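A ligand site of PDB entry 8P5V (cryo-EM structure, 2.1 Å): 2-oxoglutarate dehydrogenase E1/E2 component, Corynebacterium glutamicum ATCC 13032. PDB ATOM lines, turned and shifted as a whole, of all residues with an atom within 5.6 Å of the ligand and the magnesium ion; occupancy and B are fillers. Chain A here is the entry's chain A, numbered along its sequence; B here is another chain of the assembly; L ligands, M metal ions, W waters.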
ATOM      1  N   PHE A 512      30.682 -30.024  20.165  1.00  0.00           N
ATOM      2  CA  PHE A 512      30.365 -28.685  19.667  1.00  0.00           C
ATOM      3  C   PHE A 512      31.653 -27.917  19.368  1.00  0.00           C
ATOM      4  O   PHE A 512      31.969 -26.955  20.050  1.00  0.00           O
ATOM      5  CB  PHE A 512      29.472 -27.923  20.651  1.00  0.00           C
ATOM      6  CG  PHE A 512      28.082 -28.492  20.810  1.00  0.00           C
ATOM      7  CD1 PHE A 512      27.210 -28.501  19.735  1.00  0.00           C
ATOM      8  CD2 PHE A 512      27.663 -29.015  22.022  1.00  0.00           C
ATOM      9  CE1 PHE A 512      25.927 -29.024  19.865  1.00  0.00           C
ATOM     10  CE2 PHE A 512      26.383 -29.544  22.145  1.00  0.00           C
ATOM     11  CZ  PHE A 512      25.520 -29.551  21.071  1.00  0.00           C
ATOM     12  N   HIS A 545      27.199 -23.437  24.410  1.00  0.00           N
ATOM     13  CA  HIS A 545      27.891 -24.686  24.095  1.00  0.00           C
ATOM     14  C   HIS A 545      29.071 -24.483  23.141  1.00  0.00           C
ATOM     15  O   HIS A 545      30.091 -25.140  23.274  1.00  0.00           O
ATOM     16  CB  HIS A 545      26.902 -25.672  23.480  1.00  0.00           C
ATOM     17  CG  HIS A 545      26.210 -25.144  22.263  1.00  0.00           C
ATOM     18  ND1 HIS A 545      26.431 -25.663  21.000  1.00  0.00           N
ATOM     19  CD2 HIS A 545      25.345 -24.126  22.084  1.00  0.00           C
ATOM     20  CE1 HIS A 545      25.715 -24.989  20.120  1.00  0.00           C
ATOM     21  NE2 HIS A 545      25.046 -24.043  20.754  1.00  0.00           N
ATOM     22  N   ARG A 546      28.915 -23.589  22.152  1.00  0.00           N
ATOM     23  CA  ARG A 546      29.828 -23.513  21.025  1.00  0.00           C
ATOM     24  C   ARG A 546      31.248 -23.196  21.495  1.00  0.00           C
ATOM     25  O   ARG A 546      31.548 -22.068  21.861  1.00  0.00           O
ATOM     26  CB  ARG A 546      29.343 -22.455  20.025  1.00  0.00           C
ATOM     27  CG  ARG A 546      30.169 -22.330  18.747  1.00  0.00           C
ATOM     28  CD  ARG A 546      30.190 -23.592  17.908  1.00  0.00           C
ATOM     29  NE  ARG A 546      28.847 -23.990  17.502  1.00  0.00           N
ATOM     30  CZ  ARG A 546      28.518 -25.185  17.030  1.00  0.00           C
ATOM     31  NH1 ARG A 546      29.437 -26.098  16.806  1.00  0.00           N
ATOM     32  NH2 ARG A 546      27.244 -25.453  16.773  1.00  0.00           N
ATOM     33  N   SER A 610      21.239 -26.021  29.161  1.00  0.00           N
ATOM     34  CA  SER A 610      21.219 -26.123  27.715  1.00  0.00           C
ATOM     35  C   SER A 610      20.311 -25.048  27.099  1.00  0.00           C
ATOM     36  O   SER A 610      20.403 -24.781  25.909  1.00  0.00           O
ATOM     37  CB  SER A 610      20.788 -27.495  27.281  1.00  0.00           C
ATOM     38  OG  SER A 610      20.873 -27.618  25.868  1.00  0.00           O
ATOM     39  N   HIS A 611      19.435 -24.450  27.915  1.00  0.00           N
ATOM     40  CA  HIS A 611      18.541 -23.395  27.478  1.00  0.00           C
ATOM     41  C   HIS A 611      19.348 -22.140  27.147  1.00  0.00           C
ATOM     42  O   HIS A 611      19.897 -21.501  28.037  1.00  0.00           O
ATOM     43  CB  HIS A 611      17.498 -23.104  28.553  1.00  0.00           C
ATOM     44  CG  HIS A 611      16.528 -24.214  28.770  1.00  0.00           C
ATOM     45  ND1 HIS A 611      16.875 -25.549  28.795  1.00  0.00           N
ATOM     46  CD2 HIS A 611      15.200 -24.169  28.968  1.00  0.00           C
ATOM     47  CE1 HIS A 611      15.788 -26.273  28.991  1.00  0.00           C
ATOM     48  NE2 HIS A 611      14.763 -25.457  29.106  1.00  0.00           N
ATOM     49  N   LEU A 612      19.383 -21.778  25.861  1.00  0.00           N
ATOM     50  CA  LEU A 612      20.257 -20.723  25.374  1.00  0.00           C
ATOM     51  C   LEU A 612      19.884 -19.377  25.996  1.00  0.00           C
ATOM     52  O   LEU A 612      18.716 -19.094  26.208  1.00  0.00           O
ATOM     53  CB  LEU A 612      20.161 -20.669  23.839  1.00  0.00           C
ATOM     54  CG  LEU A 612      20.704 -21.900  23.108  1.00  0.00           C
ATOM     55  CD1 LEU A 612      20.451 -21.789  21.613  1.00  0.00           C
ATOM     56  CD2 LEU A 612      22.190 -22.086  23.373  1.00  0.00           C
ATOM     57  N   GLY A 646      25.472 -17.049  20.412  1.00  0.00           N
ATOM     58  CA  GLY A 646      25.302 -17.466  19.028  1.00  0.00           C
ATOM     59  C   GLY A 646      24.392 -16.502  18.272  1.00  0.00           C
ATOM     60  O   GLY A 646      23.550 -15.857  18.887  1.00  0.00           O
ATOM     61  N   ASP A 647      24.575 -16.421  16.950  1.00  0.00           N
ATOM     62  CA  ASP A 647      23.859 -15.445  16.132  1.00  0.00           C
ATOM     63  C   ASP A 647      22.359 -15.736  16.132  1.00  0.00           C
ATOM     64  O   ASP A 647      21.563 -14.809  16.264  1.00  0.00           O
ATOM     65  CB  ASP A 647      24.405 -15.378  14.711  1.00  0.00           C
ATOM     66  CG  ASP A 647      24.577 -16.715  14.002  1.00  0.00           C
ATOM     67  OD1 ASP A 647      24.663 -17.739  14.699  1.00  0.00           O
ATOM     68  OD2 ASP A 647      24.605 -16.716  12.765  1.00  0.00           O
ATOM     69  N   ALA A 648      21.978 -17.006  15.978  1.00  0.00           N
ATOM     70  CA  ALA A 648      20.565 -17.374  15.957  1.00  0.00           C
ATOM     71  C   ALA A 648      19.913 -17.075  17.308  1.00  0.00           C
ATOM     72  O   ALA A 648      18.825 -16.519  17.356  1.00  0.00           O
ATOM     73  CB  ALA A 648      20.388 -18.813  15.572  1.00  0.00           C
ATOM     74  N   ALA A 649      20.606 -17.433  18.397  1.00  0.00           N
ATOM     75  CA  ALA A 649      20.072 -17.247  19.730  1.00  0.00           C
ATOM     76  C   ALA A 649      20.011 -15.766  20.081  1.00  0.00           C
ATOM     77  O   ALA A 649      19.073 -15.324  20.747  1.00  0.00           O
ATOM     78  CB  ALA A 649      20.904 -18.014  20.727  1.00  0.00           C
ATOM     79  N   PHE A 650      21.021 -14.996  19.656  1.00  0.00           N
ATOM     80  CA  PHE A 650      21.099 -13.585  19.985  1.00  0.00           C
ATOM     81  C   PHE A 650      19.926 -12.852  19.337  1.00  0.00           C
ATOM     82  O   PHE A 650      19.322 -11.983  19.969  1.00  0.00           O
ATOM     83  CB  PHE A 650      22.444 -12.999  19.565  1.00  0.00           C
ATOM     84  CG  PHE A 650      22.681 -11.580  20.020  1.00  0.00           C
ATOM     85  CD1 PHE A 650      22.239 -10.496  19.268  1.00  0.00           C
ATOM     86  CD2 PHE A 650      23.296 -11.321  21.231  1.00  0.00           C
ATOM     87  CE1 PHE A 650      22.439  -9.198  19.707  1.00  0.00           C
ATOM     88  CE2 PHE A 650      23.496 -10.023  21.670  1.00  0.00           C
ATOM     89  CZ  PHE A 650      23.074  -8.963  20.905  1.00  0.00           C
ATOM     90  N   LEU A 653      16.056 -15.306  20.611  1.00  0.00           N
ATOM     91  CA  LEU A 653      15.533 -15.278  21.968  1.00  0.00           C
ATOM     92  C   LEU A 653      15.404 -13.846  22.465  1.00  0.00           C
ATOM     93  O   LEU A 653      16.184 -12.981  22.073  1.00  0.00           O
ATOM     94  CB  LEU A 653      16.446 -16.110  22.886  1.00  0.00           C
ATOM     95  CG  LEU A 653      16.379 -17.621  22.697  1.00  0.00           C
ATOM     96  CD1 LEU A 653      17.518 -18.306  23.414  1.00  0.00           C
ATOM     97  CD2 LEU A 653      15.038 -18.206  23.161  1.00  0.00           C
ATOM     98  N   VAL A 678      29.165 -14.928  18.184  1.00  0.00           N
ATOM     99  CA  VAL A 678      29.838 -15.834  17.274  1.00  0.00           C
ATOM    100  C   VAL A 678      28.913 -16.049  16.085  1.00  0.00           C
ATOM    101  O   VAL A 678      28.049 -16.922  16.110  1.00  0.00           O
ATOM    102  CB  VAL A 678      30.218 -17.156  17.967  1.00  0.00           C
ATOM    103  CG1 VAL A 678      30.940 -18.106  17.018  1.00  0.00           C
ATOM    104  CG2 VAL A 678      31.045 -16.917  19.209  1.00  0.00           C
ATOM    105  N   ASN A 679      29.096 -15.219  15.049  1.00  0.00           N
ATOM    106  CA  ASN A 679      28.225 -15.228  13.888  1.00  0.00           C
ATOM    107  C   ASN A 679      28.770 -16.222  12.867  1.00  0.00           C
ATOM    108  O   ASN A 679      29.496 -15.847  11.958  1.00  0.00           O
ATOM    109  CB  ASN A 679      28.091 -13.807  13.330  1.00  0.00           C
ATOM    110  CG  ASN A 679      27.114 -13.707  12.182  1.00  0.00           C
ATOM    111  OD1 ASN A 679      26.413 -14.671  11.874  1.00  0.00           O
ATOM    112  ND2 ASN A 679      27.064 -12.548  11.559  1.00  0.00           N
ATOM    113  N   ASN A 680      28.392 -17.500  13.020  1.00  0.00           N
ATOM    114  CA  ASN A 680      28.802 -18.541  12.088  1.00  0.00           C
ATOM    115  C   ASN A 680      27.755 -18.695  10.979  1.00  0.00           C
ATOM    116  O   ASN A 680      27.833 -19.633  10.203  1.00  0.00           O
ATOM    117  CB  ASN A 680      29.084 -19.861  12.811  1.00  0.00           C
ATOM    118  CG  ASN A 680      27.938 -20.326  13.681  1.00  0.00           C
ATOM    119  OD1 ASN A 680      26.857 -19.731  13.666  1.00  0.00           O
ATOM    120  ND2 ASN A 680      28.168 -21.374  14.444  1.00  0.00           N
ATOM    121  N   GLN A 681      26.792 -17.765  10.942  1.00  0.00           N
ATOM    122  CA  GLN A 681      25.895 -17.590   9.814  1.00  0.00           C
ATOM    123  C   GLN A 681      24.941 -18.775   9.680  1.00  0.00           C
ATOM    124  O   GLN A 681      24.448 -19.035   8.577  1.00  0.00           O
ATOM    125  CB  GLN A 681      26.695 -17.369   8.522  1.00  0.00           C
ATOM    126  CG  GLN A 681      27.684 -16.218   8.616  1.00  0.00           C
ATOM    127  CD  GLN A 681      28.471 -16.030   7.336  1.00  0.00           C
ATOM    128  OE1 GLN A 681      27.923 -15.623   6.316  1.00  0.00           O
ATOM    129  NE2 GLN A 681      29.765 -16.292   7.396  1.00  0.00           N
ATOM    130  N   ILE A 682      24.666 -19.462  10.789  1.00  0.00           N
ATOM    131  CA  ILE A 682      23.768 -20.609  10.785  1.00  0.00           C
ATOM    132  C   ILE A 682      23.381 -20.948  12.221  1.00  0.00           C
ATOM    133  O   ILE A 682      24.132 -20.671  13.157  1.00  0.00           O
ATOM    134  CB  ILE A 682      24.416 -21.810  10.067  1.00  0.00           C
ATOM    135  CG1 ILE A 682      23.373 -22.872   9.699  1.00  0.00           C
ATOM    136  CG2 ILE A 682      25.555 -22.400  10.894  1.00  0.00           C
ATOM    137  CD1 ILE A 682      23.908 -23.950   8.780  1.00  0.00           C
ATOM    138  N   GLY A 683      22.197 -21.538  12.383  1.00  0.00           N
ATOM    139  CA  GLY A 683      21.763 -22.139  13.632  1.00  0.00           C
ATOM    140  C   GLY A 683      22.082 -23.629  13.648  1.00  0.00           C
ATOM    141  O   GLY A 683      23.235 -24.034  13.500  1.00  0.00           O
ATOM    142  N   PHE A 684      21.047 -24.457  13.832  1.00  0.00           N
ATOM    143  CA  PHE A 684      21.153 -25.889  13.667  1.00  0.00           C
ATOM    144  C   PHE A 684      21.131 -26.182  12.170  1.00  0.00           C
ATOM    145  O   PHE A 684      22.116 -26.655  11.608  1.00  0.00           O
ATOM    146  CB  PHE A 684      20.054 -26.591  14.461  1.00  0.00           C
ATOM    147  CG  PHE A 684      20.175 -28.079  14.624  1.00  0.00           C
ATOM    148  CD1 PHE A 684      20.401 -28.914  13.528  1.00  0.00           C
ATOM    149  CD2 PHE A 684      20.020 -28.667  15.872  1.00  0.00           C
ATOM    150  CE1 PHE A 684      20.488 -30.287  13.698  1.00  0.00           C
ATOM    151  CE2 PHE A 684      20.119 -30.037  16.029  1.00  0.00           C
ATOM    152  CZ  PHE A 684      20.338 -30.851  14.940  1.00  0.00           C
ATOM    153  N   ARG A 745      30.809 -22.349  10.534  1.00  0.00           N
ATOM    154  CA  ARG A 745      30.784 -23.596  11.280  1.00  0.00           C
ATOM    155  C   ARG A 745      31.227 -24.715  10.348  1.00  0.00           C
ATOM    156  O   ARG A 745      30.489 -25.083   9.432  1.00  0.00           O
ATOM    157  CB  ARG A 745      29.371 -23.819  11.820  1.00  0.00           C
ATOM    158  CG  ARG A 745      29.248 -24.977  12.800  1.00  0.00           C
ATOM    159  CD  ARG A 745      27.796 -25.394  12.950  1.00  0.00           C
ATOM    160  NE  ARG A 745      27.292 -25.996  11.718  1.00  0.00           N
ATOM    161  CZ  ARG A 745      26.013 -26.148  11.407  1.00  0.00           C
ATOM    162  NH1 ARG A 745      25.057 -25.705  12.207  1.00  0.00           N
ATOM    163  NH2 ARG A 745      25.687 -26.758  10.282  1.00  0.00           N
ATOM    164  N   HIS A 749      25.922 -29.095  13.076  1.00  0.00           N
ATOM    165  CA  HIS A 749      25.604 -28.501  14.358  1.00  0.00           C
ATOM    166  C   HIS A 749      26.362 -29.238  15.454  1.00  0.00           C
ATOM    167  O   HIS A 749      27.029 -28.617  16.280  1.00  0.00           O
ATOM    168  CB  HIS A 749      24.088 -28.517  14.595  1.00  0.00           C
ATOM    169  CG  HIS A 749      23.708 -27.941  15.912  1.00  0.00           C
ATOM    170  ND1 HIS A 749      23.143 -28.704  16.918  1.00  0.00           N
ATOM    171  CD2 HIS A 749      23.833 -26.701  16.404  1.00  0.00           C
ATOM    172  CE1 HIS A 749      22.918 -27.927  17.970  1.00  0.00           C
ATOM    173  NE2 HIS A 749      23.333 -26.711  17.676  1.00  0.00           N
ATOM    174  N   GLU B 903      11.483 -26.047  14.673  1.00  0.00           N
ATOM    175  CA  GLU B 903      12.909 -25.931  14.422  1.00  0.00           C
ATOM    176  C   GLU B 903      13.386 -27.188  13.689  1.00  0.00           C
ATOM    177  O   GLU B 903      13.267 -28.299  14.215  1.00  0.00           O
ATOM    178  CB  GLU B 903      13.657 -25.708  15.733  1.00  0.00           C
ATOM    179  CG  GLU B 903      13.356 -24.363  16.370  1.00  0.00           C
ATOM    180  CD  GLU B 903      13.885 -24.189  17.781  1.00  0.00           C
ATOM    181  OE1 GLU B 903      14.517 -25.136  18.297  1.00  0.00           O
ATOM    182  OE2 GLU B 903      13.663 -23.101  18.374  1.00  0.00           O
ATOM    183  N   ASP B 904      13.869 -26.992  12.465  1.00  0.00           N
ATOM    184  CA  ASP B 904      14.486 -28.047  11.671  1.00  0.00           C
ATOM    185  C   ASP B 904      13.443 -29.109  11.303  1.00  0.00           C
ATOM    186  O   ASP B 904      13.759 -30.299  11.251  1.00  0.00           O
ATOM    187  CB  ASP B 904      15.683 -28.650  12.404  1.00  0.00           C
ATOM    188  CG  ASP B 904      16.656 -27.601  12.927  1.00  0.00           C
ATOM    189  OD1 ASP B 904      17.658 -27.340  12.232  1.00  0.00           O
ATOM    190  OD2 ASP B 904      16.405 -27.045  14.017  1.00  0.00           O
ATOM    191  N   LEU B 949      14.692 -19.528  15.874  1.00  0.00           N
ATOM    192  CA  LEU B 949      15.142 -20.016  17.171  1.00  0.00           C
ATOM    193  C   LEU B 949      14.266 -19.396  18.252  1.00  0.00           C
ATOM    194  O   LEU B 949      14.618 -18.372  18.848  1.00  0.00           O
ATOM    195  CB  LEU B 949      16.621 -19.615  17.330  1.00  0.00           C
ATOM    196  CG  LEU B 949      17.456 -20.403  18.348  1.00  0.00           C
ATOM    197  CD1 LEU B 949      16.926 -20.231  19.766  1.00  0.00           C
ATOM    198  CD2 LEU B 949      17.505 -21.873  17.982  1.00  0.00           C
ATOM    199  N   GLU B 951      10.778 -20.755  21.005  1.00  0.00           N
ATOM    200  CA  GLU B 951       9.680 -21.616  21.423  1.00  0.00           C
ATOM    201  C   GLU B 951       8.467 -20.759  21.766  1.00  0.00           C
ATOM    202  O   GLU B 951       7.357 -21.090  21.362  1.00  0.00           O
ATOM    203  CB  GLU B 951      10.092 -22.475  22.622  1.00  0.00           C
ATOM    204  CG  GLU B 951      11.063 -23.585  22.275  1.00  0.00           C
ATOM    205  CD  GLU B 951      12.487 -23.132  22.023  1.00  0.00           C
ATOM    206  OE1 GLU B 951      13.012 -22.331  22.824  1.00  0.00           O
ATOM    207  OE2 GLU B 951      13.085 -23.588  21.022  1.00  0.00           O
ATOM    208  N   GLN B 975      12.186 -29.183  18.989  1.00  0.00           N
ATOM    209  CA  GLN B 975      13.394 -29.917  18.657  1.00  0.00           C
ATOM    210  C   GLN B 975      13.575 -31.025  19.683  1.00  0.00           C
ATOM    211  O   GLN B 975      13.787 -32.184  19.320  1.00  0.00           O
ATOM    212  CB  GLN B 975      14.583 -28.958  18.610  1.00  0.00           C
ATOM    213  CG  GLN B 975      15.841 -29.610  18.038  1.00  0.00           C
ATOM    214  CD  GLN B 975      16.634 -28.629  17.218  1.00  0.00           C
ATOM    215  OE1 GLN B 975      16.996 -27.549  17.696  1.00  0.00           O
ATOM    216  NE2 GLN B 975      16.898 -28.973  15.967  1.00  0.00           N
ATOM    217  N   PHE B 979      12.695 -28.283  25.722  1.00  0.00           N
ATOM    218  CA  PHE B 979      12.764 -26.858  25.452  1.00  0.00           C
ATOM    219  C   PHE B 979      11.370 -26.220  25.415  1.00  0.00           C
ATOM    220  O   PHE B 979      11.267 -25.006  25.316  1.00  0.00           O
ATOM    221  CB  PHE B 979      13.491 -26.591  24.132  1.00  0.00           C
ATOM    222  CG  PHE B 979      14.900 -27.136  24.088  1.00  0.00           C
ATOM    223  CD1 PHE B 979      15.815 -26.791  25.068  1.00  0.00           C
ATOM    224  CD2 PHE B 979      15.299 -27.988  23.076  1.00  0.00           C
ATOM    225  CE1 PHE B 979      17.109 -27.302  25.033  1.00  0.00           C
ATOM    226  CE2 PHE B 979      16.592 -28.500  23.041  1.00  0.00           C
ATOM    227  CZ  PHE B 979      17.494 -28.150  24.027  1.00  0.00           C
HETATM  228  N1  LIG L   1      15.931 -23.609  22.143  1.00  0.00           N
HETATM  229  C1  LIG L   1      16.529 -23.260  23.291  1.00  0.00           C
HETATM  230  C2  LIG L   1      15.901 -22.164  24.085  1.00  0.00           C
HETATM  231  N2  LIG L   1      17.656 -23.800  23.784  1.00  0.00           N
HETATM  232  C3  LIG L   1      18.249 -24.774  23.075  1.00  0.00           C
HETATM  233  N3  LIG L   1      19.308 -25.363  23.629  1.00  0.00           N
HETATM  234  C4  LIG L   1      17.700 -25.212  21.830  1.00  0.00           C
HETATM  235  C5  LIG L   1      16.534 -24.588  21.443  1.00  0.00           C
HETATM  236  C6  LIG L   1      18.364 -26.253  20.957  1.00  0.00           C
HETATM  237  N4  LIG L   1      19.626 -25.764  20.351  1.00  0.00           N
HETATM  238  C7  LIG L   1      20.807 -25.898  20.902  1.00  0.00           C
HETATM  239  S1  LIG L   1      22.016 -25.165  20.008  1.00  0.00           S
HETATM  240  C8  LIG L   1      20.892 -24.650  18.831  1.00  0.00           C
HETATM  241  C9  LIG L   1      19.635 -25.056  19.147  1.00  0.00           C
HETATM  242  C10 LIG L   1      18.396 -24.863  18.349  1.00  0.00           C
HETATM  243  C11 LIG L   1      21.325 -23.822  17.654  1.00  0.00           C
HETATM  244  C12 LIG L   1      21.459 -22.351  17.978  1.00  0.00           C
HETATM  245  O1  LIG L   1      22.285 -21.726  16.962  1.00  0.00           O
HETATM  246  P1  LIG L   1      23.159 -20.433  17.304  1.00  0.00           P
HETATM  247  O2  LIG L   1      23.449 -19.697  16.057  1.00  0.00           O
HETATM  248  O3  LIG L   1      22.549 -19.694  18.422  1.00  0.00           O
HETATM  249  O4  LIG L   1      24.499 -21.140  17.823  1.00  0.00           O
HETATM  250  P2  LIG L   1      25.576 -22.071  17.083  1.00  0.00           P
HETATM  251  O5  LIG L   1      25.482 -21.760  15.608  1.00  0.00           O
HETATM  252  O6  LIG L   1      26.891 -21.639  17.701  1.00  0.00           O
HETATM  253  O7  LIG L   1      25.220 -23.506  17.403  1.00  0.00           O
HETATM  254 MG    MG M   1      25.125 -19.835  14.707  1.00  0.00          MG
HETATM  255  O   HOH W   1      23.975 -19.981  20.785  1.00  0.00           O
HETATM  256  O   HOH W   2      26.658 -20.725  20.182  1.00  0.00           O
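The magnesium ion is bound by O of Ile 682 (2.0 Å), OD1 of Asn 680 (2.0 Å), OD1 of Asp 647 (2.1 Å), O5 of the ligand (2.2 Å) and O2 of the ligand (2.2 Å).
The magnesium ion has five donor atoms within binding distance.
Water W1 lies within hydrogen-bond range of O3 of the ligand (2.8 Å) and N of Gly 646 (3.3 Å).
Within 4 Å of the magnesium ion: Asp 647, Asn 680 and Ile 682.
A nitrogen (N1) of the ligand sits close to the side-chain carboxylate (OE2) of Glu 951 of chain B (3.1 Å).
CA of His 611 touches N2 of the ligand (3.8 Å).
Gly 646 touches the ligand.
Gly 683 touches the ligand (CA to O1, 3.4 Å).
Phe 684 touches the ligand.
Glu 903 of chain B touches the ligand (OE1 to C5, 3.8 Å).
Leu 949 of chain B touches the ligand (CD2 to C10, 3.1 Å).
OE1 of Gln 975 of chain B touches C10 of the ligand (3.1 Å).
CE1 of Phe 979 of chain B touches N3 of the ligand, at 3.3 Å.
Hydrophobic or aromatic side chains that line the ligand: His 545, Leu 612, Ala 648, Ala 649, His 749, Leu 949 of chain B and Phe 979 of chain B.
Of the 27 residues printed, 19 come within 4 Å of the ligand.
The backbone carbonyl oxygen of Phe 684 is in hydrogen-bond range of the guanidinium group of Arg 745, 3.1 Å away.
O of Gly 683 is in hydrogen-bond range of NH1 of Arg 745 (2.8 Å).
The side-chain carboxylate (OD2) of Asp 647 is in hydrogen-bond range of the backbone NH (N) of Gln 681.
The side-chain carboxylate (OD2) of Asp 647 lies close to the side-chain amide oxygen (OD1) of Asn 679 (2.9 Å).
NE2 of Gln 975 of chain B sits at hydrogen-bond distance from OD2 of Asp 904 of chain B (2.8 Å).
The backbone carbonyl oxygen (O) of His 749 lies within hydrogen-bond range of the guanidinium group (NH2) of Arg 546 (3.2 Å).
The backbone NH (N) of Ala 648 sits close to an oxygen (O2) of the ligand (3.1 Å).
A ring nitrogen (NE2) of His 749 lies close to a sulfur (S1) of the ligand (3.1 Å).
O3 of the ligand is in hydrogen-bond range of N of Ala 649 (3.0 Å).
The guanidinium group (NH2) of Arg 546 lies within salt-bridge range of an oxygen (O7) of the ligand (2.9 Å).
A ring nitrogen (NE2) of His 545 lies close to a sulfur (S1) of the ligand, at 3.3 Å.
The backbone carbonyl oxygen of Ser 610 is in hydrogen-bond range of a nitrogen (N3) of the ligand (2.6 Å).
The backbone NH (N) of Leu 612 is in hydrogen-bond range of a nitrogen (N2) of the ligand, at 3.4 Å.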
